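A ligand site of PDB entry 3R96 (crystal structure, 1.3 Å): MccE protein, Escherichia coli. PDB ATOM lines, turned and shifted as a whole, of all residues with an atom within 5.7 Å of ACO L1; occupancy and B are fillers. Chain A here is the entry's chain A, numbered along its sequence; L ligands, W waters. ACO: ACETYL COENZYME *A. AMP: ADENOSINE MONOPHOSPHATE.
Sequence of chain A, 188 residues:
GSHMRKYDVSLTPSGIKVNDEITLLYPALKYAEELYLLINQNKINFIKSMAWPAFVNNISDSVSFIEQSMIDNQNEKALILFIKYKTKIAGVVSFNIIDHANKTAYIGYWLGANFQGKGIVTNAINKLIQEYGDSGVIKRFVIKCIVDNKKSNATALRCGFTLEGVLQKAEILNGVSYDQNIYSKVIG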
ATOM      1  N   PHE A  46      32.567  -6.445  16.354  1.00  0.00           N
ATOM      2  CA  PHE A  46      32.722  -5.887  17.699  1.00  0.00           C
ATOM      3  C   PHE A  46      34.058  -5.186  17.909  1.00  0.00           C
ATOM      4  O   PHE A  46      34.146  -4.206  18.646  1.00  0.00           O
ATOM      5  CB  PHE A  46      32.570  -6.978  18.758  1.00  0.00           C
ATOM      6  CG  PHE A  46      31.150  -7.374  19.058  1.00  0.00           C
ATOM      7  CD1 PHE A  46      30.055  -6.769  18.425  1.00  0.00           C
ATOM      8  CD2 PHE A  46      30.915  -8.350  20.011  1.00  0.00           C
ATOM      9  CE1 PHE A  46      28.754  -7.149  18.747  1.00  0.00           C
ATOM     10  CE2 PHE A  46      29.622  -8.725  20.330  1.00  0.00           C
ATOM     11  CZ  PHE A  46      28.541  -8.121  19.701  1.00  0.00           C
ATOM     12  N   SER A  49      34.405  -1.377  17.632  1.00  0.00           N
ATOM     13  CA  SER A  49      33.892  -0.436  18.626  1.00  0.00           C
ATOM     14  C   SER A  49      34.256  -0.724  20.083  1.00  0.00           C
ATOM     15  O   SER A  49      33.944   0.075  20.960  1.00  0.00           O
ATOM     16  CB  SER A  49      32.382  -0.317  18.502  1.00  0.00           C
ATOM     17  OG  SER A  49      31.773  -1.544  18.802  1.00  0.00           O
ATOM     18  N   MET A  50      34.892  -1.863  20.347  1.00  0.00           N
ATOM     19  CA  MET A  50      35.274  -2.256  21.710  1.00  0.00           C
ATOM     20  C   MET A  50      36.661  -2.884  21.678  1.00  0.00           C
ATOM     21  O   MET A  50      37.059  -3.454  20.659  1.00  0.00           O
ATOM     22  CB  MET A  50      34.239  -3.224  22.300  1.00  0.00           C
ATOM     23  CG  MET A  50      32.824  -2.655  22.398  1.00  0.00           C
ATOM     24  SD  MET A  50      31.599  -3.783  23.092  1.00  0.00           S
ATOM     25  CE  MET A  50      31.552  -5.087  21.863  1.00  0.00           C
ATOM     26  N   ILE A 107      27.225   3.237  32.405  1.00  0.00           N
ATOM     27  CA  ILE A 107      26.556   2.153  31.679  1.00  0.00           C
ATOM     28  C   ILE A 107      27.355   1.673  30.457  1.00  0.00           C
ATOM     29  O   ILE A 107      27.957   2.469  29.743  1.00  0.00           O
ATOM     30  CB  ILE A 107      25.151   2.631  31.233  1.00  0.00           C
ATOM     31  CG1 ILE A 107      24.242   2.829  32.453  1.00  0.00           C
ATOM     32  CG2 ILE A 107      24.536   1.672  30.237  1.00  0.00           C
ATOM     33  CD1 ILE A 107      23.037   3.692  32.190  1.00  0.00           C
ATOM     34  N   GLY A 108      27.329   0.371  30.227  1.00  0.00           N
ATOM     35  CA  GLY A 108      27.875  -0.223  29.006  1.00  0.00           C
ATOM     36  C   GLY A 108      26.908  -1.247  28.443  1.00  0.00           C
ATOM     37  O   GLY A 108      26.009  -1.731  29.140  1.00  0.00           O
ATOM     38  N   TYR A 109      27.094  -1.586  27.163  1.00  0.00           N
ATOM     39  CA  TYR A 109      26.189  -2.531  26.496  1.00  0.00           C
ATOM     40  C   TYR A 109      26.755  -3.042  25.188  1.00  0.00           C
ATOM     41  O   TYR A 109      27.545  -2.357  24.527  1.00  0.00           O
ATOM     42  CB  TYR A 109      24.811  -1.900  26.248  1.00  0.00           C
ATOM     43  CG  TYR A 109      24.841  -0.449  25.807  1.00  0.00           C
ATOM     44  CD1 TYR A 109      25.116  -0.097  24.488  1.00  0.00           C
ATOM     45  CD2 TYR A 109      24.576   0.565  26.716  1.00  0.00           C
ATOM     46  CE1 TYR A 109      25.144   1.240  24.092  1.00  0.00           C
ATOM     47  CE2 TYR A 109      24.579   1.891  26.330  1.00  0.00           C
ATOM     48  CZ  TYR A 109      24.864   2.235  25.027  1.00  0.00           C
ATOM     49  OH  TYR A 109      24.879   3.565  24.674  1.00  0.00           O
ATOM     50  N   TRP A 110      26.317  -4.235  24.816  1.00  0.00           N
ATOM     51  CA  TRP A 110      26.484  -4.734  23.462  1.00  0.00           C
ATOM     52  C   TRP A 110      25.423  -5.771  23.137  1.00  0.00           C
ATOM     53  O   TRP A 110      24.899  -6.420  24.051  1.00  0.00           O
ATOM     54  CB  TRP A 110      27.879  -5.303  23.232  1.00  0.00           C
ATOM     55  CG  TRP A 110      28.288  -6.526  24.009  1.00  0.00           C
ATOM     56  CD1 TRP A 110      29.080  -6.551  25.117  1.00  0.00           C
ATOM     57  CD2 TRP A 110      28.032  -7.908  23.677  1.00  0.00           C
ATOM     58  NE1 TRP A 110      29.308  -7.851  25.523  1.00  0.00           N
ATOM     59  CE2 TRP A 110      28.682  -8.698  24.647  1.00  0.00           C
ATOM     60  CE3 TRP A 110      27.304  -8.549  22.664  1.00  0.00           C
ATOM     61  CZ2 TRP A 110      28.626 -10.098  24.634  1.00  0.00           C
ATOM     62  CZ3 TRP A 110      27.264  -9.933  22.649  1.00  0.00           C
ATOM     63  CH2 TRP A 110      27.914 -10.691  23.624  1.00  0.00           C
ATOM     64  N   LEU A 111      25.132  -5.916  21.843  1.00  0.00           N
ATOM     65  CA  LEU A 111      24.235  -6.929  21.319  1.00  0.00           C
ATOM     66  C   LEU A 111      24.835  -7.619  20.128  1.00  0.00           C
ATOM     67  O   LEU A 111      25.445  -6.972  19.275  1.00  0.00           O
ATOM     68  CB  LEU A 111      22.919  -6.294  20.861  1.00  0.00           C
ATOM     69  CG  LEU A 111      21.965  -5.755  21.914  1.00  0.00           C
ATOM     70  CD1 LEU A 111      20.859  -4.954  21.237  1.00  0.00           C
ATOM     71  CD2 LEU A 111      21.379  -6.880  22.767  1.00  0.00           C
ATOM     72  N   GLY A 112      24.617  -8.925  20.022  1.00  0.00           N
ATOM     73  CA  GLY A 112      24.947  -9.648  18.794  1.00  0.00           C
ATOM     74  C   GLY A 112      24.171  -9.044  17.635  1.00  0.00           C
ATOM     75  O   GLY A 112      23.064  -8.521  17.807  1.00  0.00           O
ATOM     76  N   PHE A 115      20.525  -9.579  17.117  1.00  0.00           N
ATOM     77  CA  PHE A 115      19.661  -9.034  18.167  1.00  0.00           C
ATOM     78  C   PHE A 115      19.515  -7.519  18.099  1.00  0.00           C
ATOM     79  O   PHE A 115      18.752  -6.929  18.884  1.00  0.00           O
ATOM     80  CB  PHE A 115      20.162  -9.500  19.543  1.00  0.00           C
ATOM     81  CG  PHE A 115      20.229 -10.978  19.682  1.00  0.00           C
ATOM     82  CD1 PHE A 115      19.087 -11.715  19.982  1.00  0.00           C
ATOM     83  CD2 PHE A 115      21.420 -11.660  19.461  1.00  0.00           C
ATOM     84  CE1 PHE A 115      19.127 -13.107  20.094  1.00  0.00           C
ATOM     85  CE2 PHE A 115      21.481 -13.041  19.578  1.00  0.00           C
ATOM     86  CZ  PHE A 115      20.328 -13.764  19.892  1.00  0.00           C
ATOM     87  N   GLN A 116      20.219  -6.893  17.173  1.00  0.00           N
ATOM     88  CA  GLN A 116      20.153  -5.443  17.004  1.00  0.00           C
ATOM     89  C   GLN A 116      18.903  -5.040  16.233  1.00  0.00           C
ATOM     90  O   GLN A 116      18.365  -5.831  15.461  1.00  0.00           O
ATOM     91  CB  GLN A 116      21.418  -4.929  16.318  1.00  0.00           C
ATOM     92  CG  GLN A 116      22.643  -5.061  17.202  1.00  0.00           C
ATOM     93  CD  GLN A 116      23.933  -4.678  16.521  1.00  0.00           C
ATOM     94  OE1 GLN A 116      23.929  -3.916  15.556  1.00  0.00           O
ATOM     95  NE2 GLN A 116      25.046  -5.183  17.025  1.00  0.00           N
ATOM     96  N   GLY A 117      18.429  -3.813  16.449  1.00  0.00           N
ATOM     97  CA  GLY A 117      17.248  -3.312  15.750  1.00  0.00           C
ATOM     98  C   GLY A 117      15.937  -3.724  16.378  1.00  0.00           C
ATOM     99  O   GLY A 117      14.882  -3.615  15.738  1.00  0.00           O
ATOM    100  N   LYS A 118      15.982  -4.181  17.625  1.00  0.00           N
ATOM    101  CA  LYS A 118      14.802  -4.689  18.324  1.00  0.00           C
ATOM    102  C   LYS A 118      14.468  -3.913  19.597  1.00  0.00           C
ATOM    103  O   LYS A 118      13.579  -4.295  20.343  1.00  0.00           O
ATOM    104  CB  LYS A 118      14.984  -6.177  18.672  1.00  0.00           C
ATOM    105  CG  LYS A 118      15.008  -7.122  17.485  1.00  0.00           C
ATOM    106  CD  LYS A 118      15.443  -8.531  17.906  1.00  0.00           C
ATOM    107  CE  LYS A 118      15.314  -9.552  16.778  1.00  0.00           C
ATOM    108  NZ  LYS A 118      13.894  -9.904  16.511  1.00  0.00           N
ATOM    109  N   GLY A 119      15.196  -2.825  19.853  1.00  0.00           N
ATOM    110  CA  GLY A 119      15.003  -2.025  21.072  1.00  0.00           C
ATOM    111  C   GLY A 119      15.413  -2.705  22.366  1.00  0.00           C
ATOM    112  O   GLY A 119      15.023  -2.281  23.445  1.00  0.00           O
ATOM    113  N   ILE A 120      16.211  -3.761  22.266  1.00  0.00           N
ATOM    114  CA  ILE A 120      16.499  -4.574  23.436  1.00  0.00           C
ATOM    115  C   ILE A 120      17.321  -3.820  24.487  1.00  0.00           C
ATOM    116  O   ILE A 120      17.024  -3.891  25.683  1.00  0.00           O
ATOM    117  CB  ILE A 120      17.186  -5.900  23.039  1.00  0.00           C
ATOM    118  CG1 ILE A 120      16.202  -6.788  22.245  1.00  0.00           C
ATOM    119  CG2 ILE A 120      17.778  -6.611  24.261  1.00  0.00           C
ATOM    120  CD1 ILE A 120      14.727  -6.748  22.621  1.00  0.00           C
ATOM    121  N   VAL A 121      18.360  -3.103  24.060  1.00  0.00           N
ATOM    122  CA  VAL A 121      19.195  -2.356  24.994  1.00  0.00           C
ATOM    123  C   VAL A 121      18.457  -1.132  25.554  1.00  0.00           C
ATOM    124  O   VAL A 121      18.530  -0.851  26.749  1.00  0.00           O
ATOM    125  CB  VAL A 121      20.560  -2.003  24.378  1.00  0.00           C
ATOM    126  CG1 VAL A 121      21.250  -0.881  25.164  1.00  0.00           C
ATOM    127  CG2 VAL A 121      21.447  -3.235  24.387  1.00  0.00           C
ATOM    128  N   THR A 122      17.709  -0.426  24.707  1.00  0.00           N
ATOM    129  CA  THR A 122      16.902   0.693  25.189  1.00  0.00           C
ATOM    130  C   THR A 122      15.911   0.229  26.274  1.00  0.00           C
ATOM    131  O   THR A 122      15.813   0.848  27.332  1.00  0.00           O
ATOM    132  CB  THR A 122      16.181   1.413  24.030  1.00  0.00           C
ATOM    133  OG1 THR A 122      17.157   2.164  23.296  1.00  0.00           O
ATOM    134  CG2 THR A 122      15.113   2.377  24.535  1.00  0.00           C
ATOM    135  N   ASN A 123      15.218  -0.881  26.023  1.00  0.00           N
ATOM    136  CA  ASN A 123      14.314  -1.426  27.033  1.00  0.00           C
ATOM    137  C   ASN A 123      15.053  -1.835  28.309  1.00  0.00           C
ATOM    138  O   ASN A 123      14.563  -1.587  29.411  1.00  0.00           O
ATOM    139  CB  ASN A 123      13.544  -2.619  26.484  1.00  0.00           C
ATOM    140  CG  ASN A 123      12.338  -2.234  25.660  1.00  0.00           C
ATOM    141  OD1 ASN A 123      11.555  -1.371  26.040  1.00  0.00           O
ATOM    142  ND2 ASN A 123      12.128  -2.963  24.562  1.00  0.00           N
ATOM    143  N   ILE A 143      26.357   7.567  30.226  1.00  0.00           N
ATOM    144  CA  ILE A 143      26.827   6.808  29.070  1.00  0.00           C
ATOM    145  C   ILE A 143      27.941   7.601  28.399  1.00  0.00           C
ATOM    146  O   ILE A 143      27.726   8.750  28.007  1.00  0.00           O
ATOM    147  CB  ILE A 143      25.695   6.530  28.061  1.00  0.00           C
ATOM    148  CG1 ILE A 143      24.669   5.562  28.672  1.00  0.00           C
ATOM    149  CG2 ILE A 143      26.279   5.995  26.741  1.00  0.00           C
ATOM    150  CD1 ILE A 143      23.367   5.453  27.880  1.00  0.00           C
ATOM    151  N   LYS A 144      29.121   6.999  28.293  1.00  0.00           N
ATOM    152  CA  LYS A 144      30.230   7.570  27.517  1.00  0.00           C
ATOM    153  C   LYS A 144      30.445   6.679  26.313  1.00  0.00           C
ATOM    154  O   LYS A 144      30.561   5.469  26.461  1.00  0.00           O
ATOM    155  CB  LYS A 144      31.537   7.536  28.308  1.00  0.00           C
ATOM    156  CG  LYS A 144      31.563   8.286  29.605  1.00  0.00           C
ATOM    157  CD  LYS A 144      32.937   8.133  30.208  1.00  0.00           C
ATOM    158  CE  LYS A 144      33.089   8.891  31.506  1.00  0.00           C
ATOM    159  NZ  LYS A 144      34.450   8.652  32.071  1.00  0.00           N
ATOM    160  N   CYS A 145      30.527   7.268  25.119  1.00  0.00           N
ATOM    161  CA  CYS A 145      30.784   6.458  23.932  1.00  0.00           C
ATOM    162  C   CYS A 145      31.494   7.275  22.882  1.00  0.00           C
ATOM    163  O   CYS A 145      31.326   8.492  22.785  1.00  0.00           O
ATOM    164  CB  CYS A 145      29.487   5.870  23.375  1.00  0.00           C
ATOM    165  SG  CYS A 145      28.270   7.098  22.938  1.00  0.00           S
ATOM    166  N   ILE A 146      32.299   6.588  22.070  1.00  0.00           N
ATOM    167  CA  ILE A 146      33.076   7.231  21.026  1.00  0.00           C
ATOM    168  C   ILE A 146      32.146   8.006  20.100  1.00  0.00           C
ATOM    169  O   ILE A 146      31.057   7.545  19.753  1.00  0.00           O
ATOM    170  CB  ILE A 146      33.962   6.184  20.307  1.00  0.00           C
ATOM    171  CG1 ILE A 146      35.130   5.797  21.235  1.00  0.00           C
ATOM    172  CG2 ILE A 146      34.476   6.720  18.971  1.00  0.00           C
ATOM    173  CD1 ILE A 146      35.930   4.593  20.790  1.00  0.00           C
ATOM    174  N   ASN A 149      30.571   6.368  17.053  1.00  0.00           N
ATOM    175  CA  ASN A 149      29.776   5.159  17.262  1.00  0.00           C
ATOM    176  C   ASN A 149      28.303   5.517  17.113  1.00  0.00           C
ATOM    177  O   ASN A 149      27.632   5.867  18.087  1.00  0.00           O
ATOM    178  CB  ASN A 149      30.078   4.524  18.626  1.00  0.00           C
ATOM    179  CG  ASN A 149      29.436   3.170  18.799  1.00  0.00           C
ATOM    180  OD1 ASN A 149      28.368   2.893  18.249  1.00  0.00           O
ATOM    181  ND2 ASN A 149      30.068   2.316  19.603  1.00  0.00           N
ATOM    182  N   LYS A 151      25.389   3.923  16.445  1.00  0.00           N
ATOM    183  CA  LYS A 151      24.334   3.215  17.150  1.00  0.00           C
ATOM    184  C   LYS A 151      24.351   3.441  18.655  1.00  0.00           C
ATOM    185  O   LYS A 151      23.303   3.527  19.288  1.00  0.00           O
ATOM    186  CB  LYS A 151      24.359   1.718  16.807  1.00  0.00           C
ATOM    187  CG  LYS A 151      23.991   1.410  15.357  1.00  0.00           C
ATOM    188  CD  LYS A 151      23.609  -0.051  15.170  1.00  0.00           C
ATOM    189  CE  LYS A 151      23.301  -0.394  13.714  1.00  0.00           C
ATOM    190  NZ  LYS A 151      24.513  -0.395  12.862  1.00  0.00           N
ATOM    191  N   SER A 152      25.539   3.559  19.239  1.00  0.00           N
ATOM    192  CA  SER A 152      25.609   3.770  20.688  1.00  0.00           C
ATOM    193  C   SER A 152      25.107   5.164  21.066  1.00  0.00           C
ATOM    194  O   SER A 152      24.385   5.319  22.047  1.00  0.00           O
ATOM    195  CB  SER A 152      27.014   3.542  21.229  1.00  0.00           C
ATOM    196  OG  SER A 152      26.988   3.674  22.646  1.00  0.00           O
ATOM    197  N   ALA A 154      22.916   6.886  19.329  1.00  0.00           N
ATOM    198  CA  ALA A 154      21.475   6.834  19.132  1.00  0.00           C
ATOM    199  C   ALA A 154      20.762   6.196  20.334  1.00  0.00           C
ATOM    200  O   ALA A 154      19.721   6.675  20.755  1.00  0.00           O
ATOM    201  CB  ALA A 154      21.142   6.107  17.852  1.00  0.00           C
ATOM    202  N   THR A 155      21.342   5.123  20.868  1.00  0.00           N
ATOM    203  CA  THR A 155      20.781   4.472  22.055  1.00  0.00           C
ATOM    204  C   THR A 155      20.724   5.427  23.256  1.00  0.00           C
ATOM    205  O   THR A 155      19.696   5.518  23.943  1.00  0.00           O
ATOM    206  CB  THR A 155      21.561   3.186  22.394  1.00  0.00           C
ATOM    207  OG1 THR A 155      21.347   2.238  21.336  1.00  0.00           O
ATOM    208  CG2 THR A 155      21.121   2.582  23.724  1.00  0.00           C
ATOM    209  N   ARG A 158      17.914   7.850  22.649  1.00  0.00           N
ATOM    210  CA  ARG A 158      16.645   7.118  22.707  1.00  0.00           C
ATOM    211  C   ARG A 158      16.203   6.839  24.149  1.00  0.00           C
ATOM    212  O   ARG A 158      15.008   6.774  24.441  1.00  0.00           O
ATOM    213  CB  ARG A 158      16.793   5.787  21.939  1.00  0.00           C
ATOM    214  CG  ARG A 158      15.524   5.046  21.623  1.00  0.00           C
ATOM    215  CD  ARG A 158      15.825   3.851  20.723  1.00  0.00           C
ATOM    216  NE  ARG A 158      16.243   4.247  19.374  1.00  0.00           N
ATOM    217  CZ  ARG A 158      17.462   4.100  18.859  1.00  0.00           C
ATOM    218  NH1 ARG A 158      18.466   3.547  19.555  1.00  0.00           N
ATOM    219  NH2 ARG A 158      17.709   4.507  17.615  1.00  0.00           N
ATOM    220  N   GLU A 171      39.082   7.467  24.876  1.00  0.00           N
ATOM    221  CA  GLU A 171      38.941   6.020  24.748  1.00  0.00           C
ATOM    222  C   GLU A 171      39.901   5.476  23.702  1.00  0.00           C
ATOM    223  O   GLU A 171      39.907   5.937  22.555  1.00  0.00           O
ATOM    224  CB  GLU A 171      37.498   5.615  24.427  1.00  0.00           C
ATOM    225  CG  GLU A 171      37.313   4.110  24.468  1.00  0.00           C
ATOM    226  CD  GLU A 171      35.870   3.654  24.317  1.00  0.00           C
ATOM    227  OE1 GLU A 171      34.939   4.485  24.395  1.00  0.00           O
ATOM    228  OE2 GLU A 171      35.664   2.428  24.129  1.00  0.00           O
HETATM  229  N1A ACO L   1      11.896   0.056  21.265  1.00  0.00           N
HETATM  230  C2A ACO L   1      12.887   0.848  20.805  1.00  0.00           C
HETATM  231  N3A ACO L   1      13.484   0.624  19.619  1.00  0.00           N
HETATM  232  C4A ACO L   1      13.065  -0.412  18.846  1.00  0.00           C
HETATM  233  C5A ACO L   1      12.039  -1.239  19.297  1.00  0.00           C
HETATM  234  C6A ACO L   1      11.461  -0.991  20.523  1.00  0.00           C
HETATM  235  N6A ACO L   1      10.462  -1.791  20.957  1.00  0.00           N
HETATM  236  N7A ACO L   1      11.823  -2.190  18.370  1.00  0.00           N
HETATM  237  C8A ACO L   1      12.689  -1.954  17.362  1.00  0.00           C
HETATM  238  N9A ACO L   1      13.426  -0.866  17.639  1.00  0.00           N
HETATM  239  C1B ACO L   1      14.553  -0.403  16.792  1.00  0.00           C
HETATM  240  C2B ACO L   1      14.827   1.069  16.622  1.00  0.00           C
HETATM  241  O2B ACO L   1      14.110   1.582  15.506  1.00  0.00           O
HETATM  242  C3B ACO L   1      16.330   1.097  16.409  1.00  0.00           C
HETATM  243  O3B ACO L   1      16.659   0.594  15.104  1.00  0.00           O
HETATM  244  P3B ACO L   1      17.504   1.421  13.997  1.00  0.00           P
HETATM  245  O7A ACO L   1      17.257   0.658  12.719  1.00  0.00           O
HETATM  246  O8A ACO L   1      18.949   1.415  14.449  1.00  0.00           O
HETATM  247  O9A ACO L   1      16.906   2.800  14.022  1.00  0.00           O
HETATM  248  C4B ACO L   1      16.815   0.025  17.362  1.00  0.00           C
HETATM  249  O4B ACO L   1      15.727  -0.891  17.489  1.00  0.00           O
HETATM  250  C5B ACO L   1      17.217   0.592  18.720  1.00  0.00           C
HETATM  251  O5B ACO L   1      17.511  -0.487  19.597  1.00  0.00           O
HETATM  252  P1A ACO L   1      18.444  -0.276  20.898  1.00  0.00           P
HETATM  253  O1A ACO L   1      18.648   1.188  21.164  1.00  0.00           O
HETATM  254  O2A ACO L   1      17.931  -1.143  22.002  1.00  0.00           O
HETATM  255  O3A ACO L   1      19.881  -0.879  20.452  1.00  0.00           O
HETATM  256  P2A ACO L   1      20.408  -1.415  19.025  1.00  0.00           P
HETATM  257  O4A ACO L   1      19.710  -2.685  18.650  1.00  0.00           O
HETATM  258  O5A ACO L   1      20.416  -0.285  18.055  1.00  0.00           O
HETATM  259  O6A ACO L   1      21.909  -1.757  19.454  1.00  0.00           O
HETATM  260  CBP ACO L   1      24.155  -1.277  20.233  1.00  0.00           C
HETATM  261  CCP ACO L   1      22.826  -0.699  19.766  1.00  0.00           C
HETATM  262  CDP ACO L   1      25.102  -0.118  20.528  1.00  0.00           C
HETATM  263  CEP ACO L   1      23.889  -2.091  21.505  1.00  0.00           C
HETATM  264  CAP ACO L   1      24.713  -2.168  19.119  1.00  0.00           C
HETATM  265  OAP ACO L   1      24.843  -1.393  17.928  1.00  0.00           O
HETATM  266  C9P ACO L   1      26.022  -2.838  19.444  1.00  0.00           C
HETATM  267  O9P ACO L   1      26.075  -3.784  20.223  1.00  0.00           O
HETATM  268  N8P ACO L   1      27.128  -2.362  18.868  1.00  0.00           N
HETATM  269  C7P ACO L   1      28.498  -2.872  19.003  1.00  0.00           C
HETATM  270  C6P ACO L   1      28.998  -2.773  20.437  1.00  0.00           C
HETATM  271  C5P ACO L   1      29.011  -1.333  20.895  1.00  0.00           C
HETATM  272  O5P ACO L   1      29.353  -0.427  20.149  1.00  0.00           O
HETATM  273  N4P ACO L   1      28.624  -1.094  22.148  1.00  0.00           N
HETATM  274  C3P ACO L   1      28.550   0.212  22.787  1.00  0.00           C
HETATM  275  C2P ACO L   1      29.931   0.614  23.319  1.00  0.00           C
HETATM  276  S1P ACO L   1      29.791   2.186  24.107  1.00  0.00           S
HETATM  277  C   ACO L   1      28.971   1.800  25.542  1.00  0.00           C
HETATM  278  O   ACO L   1      28.829   0.646  25.943  1.00  0.00           O
HETATM  279  CH3 ACO L   1      28.380   2.925  26.346  1.00  0.00           C
HETATM  280  P   AMP L   2      33.104  -1.391  26.793  1.00  0.00           P
HETATM  281  O1P AMP L   2      33.889  -0.912  27.995  1.00  0.00           O
HETATM  282  O2P AMP L   2      32.509  -0.223  26.017  1.00  0.00           O
HETATM  283  O3P AMP L   2      33.797  -2.401  25.932  1.00  0.00           O
HETATM  284  O5' AMP L   2      31.887  -2.163  27.517  1.00  0.00           O
HETATM  285  C5' AMP L   2      30.737  -2.474  26.739  1.00  0.00           C
HETATM  286  C4' AMP L   2      30.086  -3.753  27.275  1.00  0.00           C
HETATM  287  O4' AMP L   2      30.947  -4.878  27.057  1.00  0.00           O
HETATM  288  C3' AMP L   2      29.757  -3.717  28.761  1.00  0.00           C
HETATM  289  O3' AMP L   2      28.403  -4.167  28.883  1.00  0.00           O
HETATM  290  C2' AMP L   2      30.731  -4.710  29.368  1.00  0.00           C
HETATM  291  O2' AMP L   2      30.245  -5.348  30.552  1.00  0.00           O
HETATM  292  C1' AMP L   2      30.895  -5.688  28.229  1.00  0.00           C
HETATM  293  N9  AMP L   2      32.116  -6.514  28.291  1.00  0.00           N
HETATM  294  C8  AMP L   2      33.352  -6.086  28.616  1.00  0.00           C
HETATM  295  N7  AMP L   2      34.236  -7.094  28.577  1.00  0.00           N
HETATM  296  C5  AMP L   2      33.561  -8.190  28.217  1.00  0.00           C
HETATM  297  C6  AMP L   2      33.892  -9.604  27.993  1.00  0.00           C
HETATM  298  N6  AMP L   2      35.162 -10.026  28.150  1.00  0.00           N
HETATM  299  N1  AMP L   2      32.896 -10.436  27.646  1.00  0.00           N
HETATM  300  C2  AMP L   2      31.628  -9.999  27.483  1.00  0.00           C
HETATM  301  N3  AMP L   2      31.250  -8.718  27.678  1.00  0.00           N
HETATM  302  C4  AMP L   2      32.166  -7.806  28.030  1.00  0.00           C
HETATM  303  O   HOH W   1      21.123   1.947  12.713  1.00  0.00           O
HETATM  304  O   HOH W   2      20.883   2.358  18.263  1.00  0.00           O
HETATM  305  O   HOH W   3       9.826  -4.479  20.718  1.00  0.00           O
HETATM  306  O   HOH W   4      26.125  -2.240  15.545  1.00  0.00           O
HETATM  307  O   HOH W   5      19.996  -0.873  15.488  1.00  0.00           O
HETATM  308  O   HOH W   6      14.184   0.132  13.184  1.00  0.00           O
HETATM  309  O   HOH W   7      19.998   3.459  15.945  1.00  0.00           O
HETATM  310  O   HOH W   8      28.047   0.202  17.393  1.00  0.00           O
HETATM  311  O   HOH W   9      30.879  -2.755  16.459  1.00  0.00           O
HETATM  312  O   HOH W  10       9.558  -3.898  23.564  1.00  0.00           O
HETATM  313  O   HOH W  11      17.805  -1.952  12.203  1.00  0.00           O
HETATM  314  O   HOH W  12      17.863  -4.412  19.771  1.00  0.00           O
HETATM  315  O   HOH W  13      14.962   4.290  15.639  1.00  0.00           O
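The side-chain amide nitrogen (NE2) of Gln 116 lies within hydrogen-bond range of the backbone carbonyl oxygen (O) of Leu 111, 2.9 Å away. OD1 of Asn 149 is in hydrogen-bond range of N of Ser 152, 3.1 Å away. OH of Tyr 109 lies within hydrogen-bond range of OG of Ser 152, at 2.9 Å. OG1 of Thr 155 sits at hydrogen-bond distance from O of Lys 151. The backbone carbonyl oxygen (O) of Gly 119 is in hydrogen-bond range of the side-chain amide nitrogen (ND2) of Asn 123 (3.2 Å). OG of Ser 152 sits close to SG of Cys 145.
Merely in contact with ACO L1: Gln 116 (3.2 Å), Lys 151 (3.3 Å), Gly 108 (3.3 Å), Lys 144 (3.4 Å), Trp 110 (3.4 Å), Ile 107 (3.5 Å), Met 50 (3.7 Å), Ile 143 (3.7 Å) and Cys 145 (3.8 Å). Hydrophobic or aromatic side chains that line ACO L1: Met 50, Tyr 109, Trp 110, Leu 111, Val 121 and Ile 143. 22 residues have an atom within 4 Å of ACO L1: Ser 49, Met 50, Ile 107, Gly 108, Tyr 109, Trp 110, Leu 111, Gln 116, Gly 117, Lys 118, Gly 119, Ile 120, Val 121, Thr 122, Ile 143, Lys 144, Cys 145, Asn 149, Lys 151, Ser 152, Thr 155 and Arg 158.
N of Thr 122 sits at hydrogen-bond distance from O2A of ACO L1, at 2.8 Å. OG1 of Thr 122 sits at hydrogen-bond distance from O1A of ACO L1 (2.8 Å). The backbone NH (N) of Gly 117 is in hydrogen-bond range of an oxygen (O4A) of ACO L1, 2.8 Å away. N of Leu 111 is in hydrogen-bond range of O9P of ACO L1 (2.8 Å). The guanidinium group (NH1) of Arg 158 lies within salt-bridge range of an oxygen (O1A) of ACO L1 (2.9 Å). The backbone NH of Val 121 lies within hydrogen-bond range of an oxygen (O2A) of ACO L1. ND2 of Asn 149 is in hydrogen-bond range of O5P of ACO L1 (2.9 Å). N of Tyr 109 sits at hydrogen-bond distance from O of ACO L1 (3.1 Å). A nitrogen (N4P) of ACO L1 lies within hydrogen-bond range of the backbone carbonyl oxygen of Tyr 109. An oxygen (O1A) of ACO L1 sits at hydrogen-bond distance from the side-chain hydroxyl (OG1) of Thr 155 (2.9 Å). An oxygen (O4B) of ACO L1 lies within hydrogen-bond range of the backbone NH of Gly 119 (3.1 Å). The side-chain hydroxyl of Ser 49 is in hydrogen-bond range of an oxygen (O5P) of ACO L1 (3.0 Å). An oxygen (O2A) of ACO L1 sits at hydrogen-bond distance from the backbone NH of Ile 120 (3.1 Å). N of Lys 118 sits at hydrogen-bond distance from O4B of ACO L1 (3.3 Å). S1P of ACO L1 lies close to OG of Ser 152 (3.5 Å). N of Tyr 109 lies within hydrogen-bond range of O3' of AMP L2 (3.4 Å). The backbone carbonyl oxygen of Gly 108 sits close to an oxygen (O3') of AMP L2, at 3.4 Å. NE1 of Trp 110 is in hydrogen-bond range of N3 of AMP L2.
Water W5 bridges O5A of ACO L1 and N of Gly 117. Water W2 lies within hydrogen-bond range of O5A of ACO L1, O of Lys 151, NH1 of Arg 158 and OG1 of Thr 155. Water W7 lies within hydrogen-bond range of an oxygen (O8A) of ACO L1 (2.7 Å) and the guanidinium group of Arg 158 (3.0 Å). Water W4 bridges OE1 of Gln 116 and OAP of ACO L1. Water W13 lies within hydrogen-bond range of O2B of ACO L1 (2.8 Å) and NH2 of Arg 158 (3.4 Å). Water W10 lies within hydrogen-bond range of ND2 of Asn 123 and N6A of ACO L1.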
